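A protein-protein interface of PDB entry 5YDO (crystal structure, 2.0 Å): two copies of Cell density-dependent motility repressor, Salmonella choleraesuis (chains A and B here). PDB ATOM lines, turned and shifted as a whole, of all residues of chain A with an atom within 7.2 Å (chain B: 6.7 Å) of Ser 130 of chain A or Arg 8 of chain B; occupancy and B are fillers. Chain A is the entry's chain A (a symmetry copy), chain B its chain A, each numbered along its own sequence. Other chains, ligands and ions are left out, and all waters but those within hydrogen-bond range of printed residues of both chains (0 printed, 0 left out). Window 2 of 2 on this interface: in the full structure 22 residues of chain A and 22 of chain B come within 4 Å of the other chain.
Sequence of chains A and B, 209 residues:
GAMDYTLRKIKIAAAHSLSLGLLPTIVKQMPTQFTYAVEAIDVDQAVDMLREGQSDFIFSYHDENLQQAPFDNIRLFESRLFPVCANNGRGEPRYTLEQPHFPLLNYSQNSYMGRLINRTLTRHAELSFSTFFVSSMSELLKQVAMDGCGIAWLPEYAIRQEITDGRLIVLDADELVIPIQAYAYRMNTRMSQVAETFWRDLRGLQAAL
The backbone NH (N) of Tyr 36 of chain B lies within hydrogen-bond range of the backbone carbonyl oxygen (O) of Phe 132 of chain A.
The backbone carbonyl oxygen (O) of Phe 102 of chain A sits at hydrogen-bond distance from the backbone NH (N) of Ser 130 of chain A. The side-chain hydroxyl (OG1) of Thr 6 of chain B sits close to the backbone NH (N) of Arg 8 of chain B, at 3.2 Å. The backbone NH (N) of Leu 104 of chain A lies within hydrogen-bond range of the backbone carbonyl oxygen (O) of Ser 130 of chain A. O of Leu 104 of chain A sits at hydrogen-bond distance from N of Phe 132 of chain A. The backbone NH (N) of Ile 10 of chain B lies within hydrogen-bond range of the backbone carbonyl oxygen (O) of Thr 35 of chain B (2.7 Å). N of Thr 35 of chain B sits at hydrogen-bond distance from O of Arg 8 of chain B, 3.0 Å away.
Arg 8 of chain B touches Ser 130 of chain A (NH2 to OG, 3.5 Å). Thr 35 of chain B touches Thr 131 of chain A (CG2 to O, 3.6 Å). Phe 34 of chain B touches Phe 132 of chain A (O to CE1, 3.2 Å). Thr 35 of chain B touches Phe 132 of chain A. CA of Phe 133 of chain A touches O of Tyr 36 of chain B, 3.4 Å away.
Ser 130 of chain A touches one residue of chain B. Arg 8 of chain B touches just one residue of chain A: Ser 130 (3.5 Å). Of the printed residues of chain A, Phe 34 of chain B touches Phe 132. Printed residues of chain A within 4 Å of Thr 35 of chain B: Thr 131 and Phe 132. Printed residues of chain A within 4 Å of Tyr 36 of chain B: Phe 132 (2.9 Å) and Phe 133 (3.4 Å). Of the printed residues of chain B, Thr 131 of chain A touches Thr 35. The nearest residue of chain B that does not touch Ser 130 of chain A is Thr 35 of chain B (5.2 Å). The nearest residue of chain A that does not touch Arg 8 of chain B is Thr 131 of chain A (5.6 Å). The nearest printed residue of chain B that does not touch Thr 131 of chain A is Tyr 36 of chain B (5.4 Å).
Printed residues of chain A that touch a printed residue of chain B: Ser 130, Thr 131, Phe 132 and Phe 133. Printed residues of chain B that touch a printed residue of chain A: Arg 8, Phe 34, Thr 35 and Tyr 36. Among the printed residues, no Asp or Glu carboxylate lies within 4 Å of a Lys or Arg side-chain nitrogen of the other chain.
No position is printed for both chains. Of the 6 pairs that touch across the chains among the printed residues, none has its exchanged pair printed and touching as well.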
ATOM      1  N   GLN A  99      29.192 -17.381  -7.037  1.00  0.00           N
ATOM      2  CA  GLN A  99      27.767 -17.169  -7.248  1.00  0.00           C
ATOM      3  C   GLN A  99      26.974 -18.245  -6.511  1.00  0.00           C
ATOM      4  O   GLN A  99      27.257 -19.441  -6.679  1.00  0.00           O
ATOM      5  CB  GLN A  99      27.433 -17.199  -8.740  1.00  0.00           C
ATOM      6  CG  GLN A  99      25.945 -17.247  -9.057  1.00  0.00           C
ATOM      7  CD  GLN A  99      25.196 -16.009  -8.581  1.00  0.00           C
ATOM      8  OE1 GLN A  99      24.136 -16.111  -7.959  1.00  0.00           O
ATOM      9  NE2 GLN A  99      25.745 -14.834  -8.872  1.00  0.00           N
ATOM     10  N   PRO A 100      26.009 -17.873  -5.675  1.00  0.00           N
ATOM     11  CA  PRO A 100      25.182 -18.888  -5.009  1.00  0.00           C
ATOM     12  C   PRO A 100      24.466 -19.763  -6.025  1.00  0.00           C
ATOM     13  O   PRO A 100      23.783 -19.271  -6.927  1.00  0.00           O
ATOM     14  CB  PRO A 100      24.196 -18.054  -4.184  1.00  0.00           C
ATOM     15  CG  PRO A 100      24.901 -16.749  -3.964  1.00  0.00           C
ATOM     16  CD  PRO A 100      25.705 -16.510  -5.205  1.00  0.00           C
ATOM     17  N   HIS A 101      24.644 -21.074  -5.878  1.00  0.00           N
ATOM     18  CA  HIS A 101      24.068 -22.070  -6.778  1.00  0.00           C
ATOM     19  C   HIS A 101      24.403 -21.759  -8.239  1.00  0.00           C
ATOM     20  O   HIS A 101      23.525 -21.577  -9.085  1.00  0.00           O
ATOM     21  CB  HIS A 101      22.556 -22.189  -6.567  1.00  0.00           C
ATOM     22  CG  HIS A 101      22.182 -22.884  -5.295  1.00  0.00           C
ATOM     23  ND1 HIS A 101      22.120 -22.235  -4.082  1.00  0.00           N
ATOM     24  CD2 HIS A 101      21.871 -24.178  -5.045  1.00  0.00           C
ATOM     25  CE1 HIS A 101      21.777 -23.095  -3.140  1.00  0.00           C
ATOM     26  NE2 HIS A 101      21.622 -24.282  -3.698  1.00  0.00           N
ATOM     27  N   PHE A 102      25.703 -21.691  -8.523  1.00  0.00           N
ATOM     28  CA  PHE A 102      26.138 -21.507  -9.898  1.00  0.00           C
ATOM     29  C   PHE A 102      25.808 -22.755 -10.719  1.00  0.00           C
ATOM     30  O   PHE A 102      25.753 -23.865 -10.182  1.00  0.00           O
ATOM     31  CB  PHE A 102      27.638 -21.195  -9.967  1.00  0.00           C
ATOM     32  CG  PHE A 102      28.543 -22.362  -9.636  1.00  0.00           C
ATOM     33  CD1 PHE A 102      28.923 -23.271 -10.613  1.00  0.00           C
ATOM     34  CD2 PHE A 102      29.053 -22.516  -8.356  1.00  0.00           C
ATOM     35  CE1 PHE A 102      29.763 -24.329 -10.312  1.00  0.00           C
ATOM     36  CE2 PHE A 102      29.894 -23.570  -8.047  1.00  0.00           C
ATOM     37  CZ  PHE A 102      30.248 -24.481  -9.027  1.00  0.00           C
ATOM     38  N   PRO A 103      25.556 -22.596 -12.020  1.00  0.00           N
ATOM     39  CA  PRO A 103      25.211 -23.755 -12.859  1.00  0.00           C
ATOM     40  C   PRO A 103      26.425 -24.643 -13.093  1.00  0.00           C
ATOM     41  O   PRO A 103      27.427 -24.216 -13.676  1.00  0.00           O
ATOM     42  CB  PRO A 103      24.716 -23.115 -14.162  1.00  0.00           C
ATOM     43  CG  PRO A 103      25.398 -21.788 -14.203  1.00  0.00           C
ATOM     44  CD  PRO A 103      25.507 -21.331 -12.774  1.00  0.00           C
ATOM     45  N   LEU A 104      26.328 -25.888 -12.637  1.00  0.00           N
ATOM     46  CA  LEU A 104      27.403 -26.862 -12.772  1.00  0.00           C
ATOM     47  C   LEU A 104      27.093 -27.826 -13.909  1.00  0.00           C
ATOM     48  O   LEU A 104      25.976 -28.347 -13.999  1.00  0.00           O
ATOM     49  CB  LEU A 104      27.600 -27.636 -11.466  1.00  0.00           C
ATOM     50  CG  LEU A 104      28.577 -28.807 -11.557  1.00  0.00           C
ATOM     51  CD1 LEU A 104      29.991 -28.267 -11.679  1.00  0.00           C
ATOM     52  CD2 LEU A 104      28.445 -29.737 -10.354  1.00  0.00           C
ATOM     53  N   LEU A 105      28.083 -28.049 -14.777  1.00  0.00           N
ATOM     54  CA  LEU A 105      28.050 -29.079 -15.810  1.00  0.00           C
ATOM     55  C   LEU A 105      28.989 -30.196 -15.365  1.00  0.00           C
ATOM     56  O   LEU A 105      30.211 -30.020 -15.357  1.00  0.00           O
ATOM     57  CB  LEU A 105      28.470 -28.510 -17.161  1.00  0.00           C
ATOM     58  CG  LEU A 105      28.062 -27.061 -17.409  1.00  0.00           C
ATOM     59  CD1 LEU A 105      28.713 -26.535 -18.675  1.00  0.00           C
ATOM     60  CD2 LEU A 105      26.552 -26.973 -17.512  1.00  0.00           C
ATOM     61  N   SER A 128      28.347 -23.211  -3.510  1.00  0.00           N
ATOM     62  CA  SER A 128      27.043 -23.811  -3.742  1.00  0.00           C
ATOM     63  C   SER A 128      26.768 -23.817  -5.239  1.00  0.00           C
ATOM     64  O   SER A 128      27.078 -22.848  -5.939  1.00  0.00           O
ATOM     65  CB  SER A 128      25.934 -23.059  -2.997  1.00  0.00           C
ATOM     66  OG  SER A 128      25.954 -21.682  -3.316  1.00  0.00           O
ATOM     67  N   PHE A 129      26.195 -24.917  -5.725  1.00  0.00           N
ATOM     68  CA  PHE A 129      25.986 -25.107  -7.151  1.00  0.00           C
ATOM     69  C   PHE A 129      24.633 -25.757  -7.384  1.00  0.00           C
ATOM     70  O   PHE A 129      24.062 -26.397  -6.498  1.00  0.00           O
ATOM     71  CB  PHE A 129      27.097 -25.966  -7.773  1.00  0.00           C
ATOM     72  CG  PHE A 129      27.270 -27.294  -7.102  1.00  0.00           C
ATOM     73  CD1 PHE A 129      28.115 -27.430  -6.015  1.00  0.00           C
ATOM     74  CD2 PHE A 129      26.565 -28.404  -7.542  1.00  0.00           C
ATOM     75  CE1 PHE A 129      28.261 -28.646  -5.384  1.00  0.00           C
ATOM     76  CE2 PHE A 129      26.707 -29.622  -6.915  1.00  0.00           C
ATOM     77  CZ  PHE A 129      27.557 -29.745  -5.835  1.00  0.00           C
ATOM     78  N   SER A 130      24.121 -25.576  -8.598  1.00  0.00           N
ATOM     79  CA  SER A 130      22.941 -26.278  -9.084  1.00  0.00           C
ATOM     80  C   SER A 130      23.341 -27.040 -10.339  1.00  0.00           C
ATOM     81  O   SER A 130      23.855 -26.445 -11.292  1.00  0.00           O
ATOM     82  CB  SER A 130      21.801 -25.302  -9.377  1.00  0.00           C
ATOM     83  OG  SER A 130      20.685 -25.979  -9.927  1.00  0.00           O
ATOM     84  N   THR A 131      23.122 -28.350 -10.340  1.00  0.00           N
ATOM     85  CA  THR A 131      23.578 -29.181 -11.448  1.00  0.00           C
ATOM     86  C   THR A 131      22.640 -28.996 -12.637  1.00  0.00           C
ATOM     87  O   THR A 131      21.489 -29.447 -12.614  1.00  0.00           O
ATOM     88  CB  THR A 131      23.663 -30.639 -11.019  1.00  0.00           C
ATOM     89  OG1 THR A 131      24.445 -30.731  -9.823  1.00  0.00           O
ATOM     90  CG2 THR A 131      24.342 -31.443 -12.085  1.00  0.00           C
ATOM     91  N   PHE A 132      23.134 -28.328 -13.679  1.00  0.00           N
ATOM     92  CA  PHE A 132      22.335 -28.023 -14.859  1.00  0.00           C
ATOM     93  C   PHE A 132      22.368 -29.127 -15.908  1.00  0.00           C
ATOM     94  O   PHE A 132      21.361 -29.351 -16.594  1.00  0.00           O
ATOM     95  CB  PHE A 132      22.827 -26.721 -15.499  1.00  0.00           C
ATOM     96  CG  PHE A 132      22.134 -26.383 -16.791  1.00  0.00           C
ATOM     97  CD1 PHE A 132      20.794 -26.020 -16.794  1.00  0.00           C
ATOM     98  CD2 PHE A 132      22.816 -26.418 -17.999  1.00  0.00           C
ATOM     99  CE1 PHE A 132      20.140 -25.708 -17.976  1.00  0.00           C
ATOM    100  CE2 PHE A 132      22.164 -26.103 -19.182  1.00  0.00           C
ATOM    101  CZ  PHE A 132      20.825 -25.749 -19.168  1.00  0.00           C
ATOM    102  N   PHE A 133      23.495 -29.819 -16.038  1.00  0.00           N
ATOM    103  CA  PHE A 133      23.731 -30.726 -17.152  1.00  0.00           C
ATOM    104  C   PHE A 133      24.708 -31.796 -16.700  1.00  0.00           C
ATOM    105  O   PHE A 133      25.793 -31.466 -16.217  1.00  0.00           O
ATOM    106  CB  PHE A 133      24.291 -29.967 -18.365  1.00  0.00           C
ATOM    107  CG  PHE A 133      24.419 -30.808 -19.603  1.00  0.00           C
ATOM    108  CD1 PHE A 133      25.554 -31.574 -19.829  1.00  0.00           C
ATOM    109  CD2 PHE A 133      23.409 -30.825 -20.549  1.00  0.00           C
ATOM    110  CE1 PHE A 133      25.671 -32.349 -20.967  1.00  0.00           C
ATOM    111  CE2 PHE A 133      23.521 -31.596 -21.691  1.00  0.00           C
ATOM    112  CZ  PHE A 133      24.654 -32.359 -21.898  1.00  0.00           C
ATOM    113  N   TYR B   5      14.533 -38.127  -9.040  1.00  0.00           N
ATOM    114  CA  TYR B   5      13.486 -37.181  -9.406  1.00  0.00           C
ATOM    115  C   TYR B   5      13.825 -35.782  -8.912  1.00  0.00           C
ATOM    116  O   TYR B   5      14.158 -35.599  -7.738  1.00  0.00           O
ATOM    117  CB  TYR B   5      12.130 -37.608  -8.829  1.00  0.00           C
ATOM    118  CG  TYR B   5      11.072 -36.541  -8.983  1.00  0.00           C
ATOM    119  CD1 TYR B   5      10.300 -36.467 -10.136  1.00  0.00           C
ATOM    120  CD2 TYR B   5      10.858 -35.592  -7.985  1.00  0.00           C
ATOM    121  CE1 TYR B   5       9.342 -35.487 -10.288  1.00  0.00           C
ATOM    122  CE2 TYR B   5       9.905 -34.605  -8.135  1.00  0.00           C
ATOM    123  CZ  TYR B   5       9.150 -34.558  -9.286  1.00  0.00           C
ATOM    124  OH  TYR B   5       8.194 -33.581  -9.432  1.00  0.00           O
ATOM    125  N   THR B   6      13.712 -34.796  -9.801  1.00  0.00           N
ATOM    126  CA  THR B   6      13.608 -33.398  -9.406  1.00  0.00           C
ATOM    127  C   THR B   6      12.438 -32.776 -10.159  1.00  0.00           C
ATOM    128  O   THR B   6      11.826 -33.405 -11.026  1.00  0.00           O
ATOM    129  CB  THR B   6      14.904 -32.609  -9.671  1.00  0.00           C
ATOM    130  OG1 THR B   6      14.999 -32.270 -11.060  1.00  0.00           O
ATOM    131  CG2 THR B   6      16.134 -33.403  -9.250  1.00  0.00           C
ATOM    132  N   LEU B   7      12.111 -31.531  -9.808  1.00  0.00           N
ATOM    133  CA  LEU B   7      11.020 -30.839 -10.492  1.00  0.00           C
ATOM    134  C   LEU B   7      11.373 -30.494 -11.935  1.00  0.00           C
ATOM    135  O   LEU B   7      10.478 -30.351 -12.777  1.00  0.00           O
ATOM    136  CB  LEU B   7      10.649 -29.570  -9.724  1.00  0.00           C
ATOM    137  CG  LEU B   7       9.764 -29.741  -8.485  1.00  0.00           C
ATOM    138  CD1 LEU B   7       9.545 -28.409  -7.796  1.00  0.00           C
ATOM    139  CD2 LEU B   7       8.426 -30.367  -8.853  1.00  0.00           C
ATOM    140  N   ARG B   8      12.657 -30.357 -12.247  1.00  0.00           N
ATOM    141  CA  ARG B   8      13.068 -29.832 -13.539  1.00  0.00           C
ATOM    142  C   ARG B   8      13.888 -30.803 -14.375  1.00  0.00           C
ATOM    143  O   ARG B   8      14.180 -30.494 -15.533  1.00  0.00           O
ATOM    144  CB  ARG B   8      13.870 -28.537 -13.350  1.00  0.00           C
ATOM    145  CG  ARG B   8      13.111 -27.429 -12.633  1.00  0.00           C
ATOM    146  CD  ARG B   8      13.982 -26.187 -12.459  1.00  0.00           C
ATOM    147  NE  ARG B   8      15.160 -26.464 -11.641  1.00  0.00           N
ATOM    148  CZ  ARG B   8      16.289 -25.760 -11.679  1.00  0.00           C
ATOM    149  NH1 ARG B   8      16.408 -24.725 -12.504  1.00  0.00           N
ATOM    150  NH2 ARG B   8      17.304 -26.095 -10.891  1.00  0.00           N
ATOM    151  N   LYS B   9      14.264 -31.966 -13.846  1.00  0.00           N
ATOM    152  CA  LYS B   9      15.220 -32.814 -14.546  1.00  0.00           C
ATOM    153  C   LYS B   9      14.552 -33.507 -15.727  1.00  0.00           C
ATOM    154  O   LYS B   9      13.459 -34.070 -15.595  1.00  0.00           O
ATOM    155  CB  LYS B   9      15.844 -33.840 -13.594  1.00  0.00           C
ATOM    156  CG  LYS B   9      16.431 -35.065 -14.265  1.00  0.00           C
ATOM    157  CD  LYS B   9      17.142 -35.961 -13.248  1.00  0.00           C
ATOM    158  CE  LYS B   9      18.290 -35.219 -12.542  1.00  0.00           C
ATOM    159  NZ  LYS B   9      18.770 -35.907 -11.308  1.00  0.00           N
ATOM    160  N   ILE B  10      15.209 -33.444 -16.884  1.00  0.00           N
ATOM    161  CA  ILE B  10      14.821 -34.187 -18.077  1.00  0.00           C
ATOM    162  C   ILE B  10      15.863 -35.274 -18.302  1.00  0.00           C
ATOM    163  O   ILE B  10      17.057 -34.979 -18.442  1.00  0.00           O
ATOM    164  CB  ILE B  10      14.709 -33.270 -19.304  1.00  0.00           C
ATOM    165  CG1 ILE B  10      13.700 -32.144 -19.062  1.00  0.00           C
ATOM    166  CG2 ILE B  10      14.303 -34.073 -20.525  1.00  0.00           C
ATOM    167  CD1 ILE B  10      12.274 -32.611 -18.917  1.00  0.00           C
ATOM    168  N   THR B  32      15.164 -21.835 -20.323  1.00  0.00           N
ATOM    169  CA  THR B  32      15.948 -22.083 -19.120  1.00  0.00           C
ATOM    170  C   THR B  32      15.089 -22.649 -17.991  1.00  0.00           C
ATOM    171  O   THR B  32      15.186 -22.195 -16.846  1.00  0.00           O
ATOM    172  CB  THR B  32      16.634 -20.790 -18.666  1.00  0.00           C
ATOM    173  OG1 THR B  32      17.149 -20.955 -17.340  1.00  0.00           O
ATOM    174  CG2 THR B  32      15.651 -19.622 -18.689  1.00  0.00           C
ATOM    175  N   GLN B  33      14.262 -23.648 -18.295  1.00  0.00           N
ATOM    176  CA  GLN B  33      13.348 -24.227 -17.321  1.00  0.00           C
ATOM    177  C   GLN B  33      13.675 -25.670 -16.963  1.00  0.00           C
ATOM    178  O   GLN B  33      12.945 -26.274 -16.171  1.00  0.00           O
ATOM    179  CB  GLN B  33      11.907 -24.150 -17.840  1.00  0.00           C
ATOM    180  CG  GLN B  33      11.444 -22.742 -18.191  1.00  0.00           C
ATOM    181  CD  GLN B  33      10.279 -22.736 -19.165  1.00  0.00           C
ATOM    182  OE1 GLN B  33       9.604 -23.750 -19.355  1.00  0.00           O
ATOM    183  NE2 GLN B  33      10.037 -21.588 -19.787  1.00  0.00           N
ATOM    184  N   PHE B  34      14.746 -26.239 -17.513  1.00  0.00           N
ATOM    185  CA  PHE B  34      15.033 -27.656 -17.342  1.00  0.00           C
ATOM    186  C   PHE B  34      16.471 -27.860 -16.889  1.00  0.00           C
ATOM    187  O   PHE B  34      17.332 -26.994 -17.059  1.00  0.00           O
ATOM    188  CB  PHE B  34      14.812 -28.445 -18.644  1.00  0.00           C
ATOM    189  CG  PHE B  34      13.541 -28.095 -19.365  1.00  0.00           C
ATOM    190  CD1 PHE B  34      12.320 -28.562 -18.909  1.00  0.00           C
ATOM    191  CD2 PHE B  34      13.570 -27.305 -20.503  1.00  0.00           C
ATOM    192  CE1 PHE B  34      11.150 -28.250 -19.571  1.00  0.00           C
ATOM    193  CE2 PHE B  34      12.398 -26.987 -21.174  1.00  0.00           C
ATOM    194  CZ  PHE B  34      11.188 -27.461 -20.706  1.00  0.00           C
ATOM    195  N   THR B  35      16.713 -29.025 -16.300  1.00  0.00           N
ATOM    196  CA  THR B  35      18.054 -29.554 -16.124  1.00  0.00           C
ATOM    197  C   THR B  35      18.125 -30.903 -16.831  1.00  0.00           C
ATOM    198  O   THR B  35      17.101 -31.550 -17.079  1.00  0.00           O
ATOM    199  CB  THR B  35      18.430 -29.678 -14.639  1.00  0.00           C
ATOM    200  OG1 THR B  35      17.592 -30.651 -14.008  1.00  0.00           O
ATOM    201  CG2 THR B  35      18.271 -28.341 -13.929  1.00  0.00           C
ATOM    202  N   TYR B  36      19.338 -31.313 -17.189  1.00  0.00           N
ATOM    203  CA  TYR B  36      19.540 -32.410 -18.126  1.00  0.00           C
ATOM    204  C   TYR B  36      20.405 -33.506 -17.518  1.00  0.00           C
ATOM    205  O   TYR B  36      21.472 -33.231 -16.961  1.00  0.00           O
ATOM    206  CB  TYR B  36      20.191 -31.911 -19.416  1.00  0.00           C
ATOM    207  CG  TYR B  36      19.377 -30.890 -20.175  1.00  0.00           C
ATOM    208  CD1 TYR B  36      19.464 -29.538 -19.871  1.00  0.00           C
ATOM    209  CD2 TYR B  36      18.532 -31.279 -21.207  1.00  0.00           C
ATOM    210  CE1 TYR B  36      18.726 -28.601 -20.567  1.00  0.00           C
ATOM    211  CE2 TYR B  36      17.792 -30.351 -21.914  1.00  0.00           C
ATOM    212  CZ  TYR B  36      17.893 -29.013 -21.593  1.00  0.00           C
ATOM    213  OH  TYR B  36      17.158 -28.081 -22.290  1.00  0.00           O
ATOM    214  N   VAL B 194       6.340 -30.792 -16.651  1.00  0.00           N
ATOM    215  CA  VAL B 194       7.632 -30.295 -17.121  1.00  0.00           C
ATOM    216  C   VAL B 194       8.106 -31.084 -18.336  1.00  0.00           C
ATOM    217  O   VAL B 194       8.649 -30.511 -19.288  1.00  0.00           O
ATOM    218  CB  VAL B 194       8.669 -30.320 -15.979  1.00  0.00           C
ATOM    219  CG1 VAL B 194       8.849 -31.731 -15.424  1.00  0.00           C
ATOM    220  CG2 VAL B 194       9.998 -29.760 -16.453  1.00  0.00           C
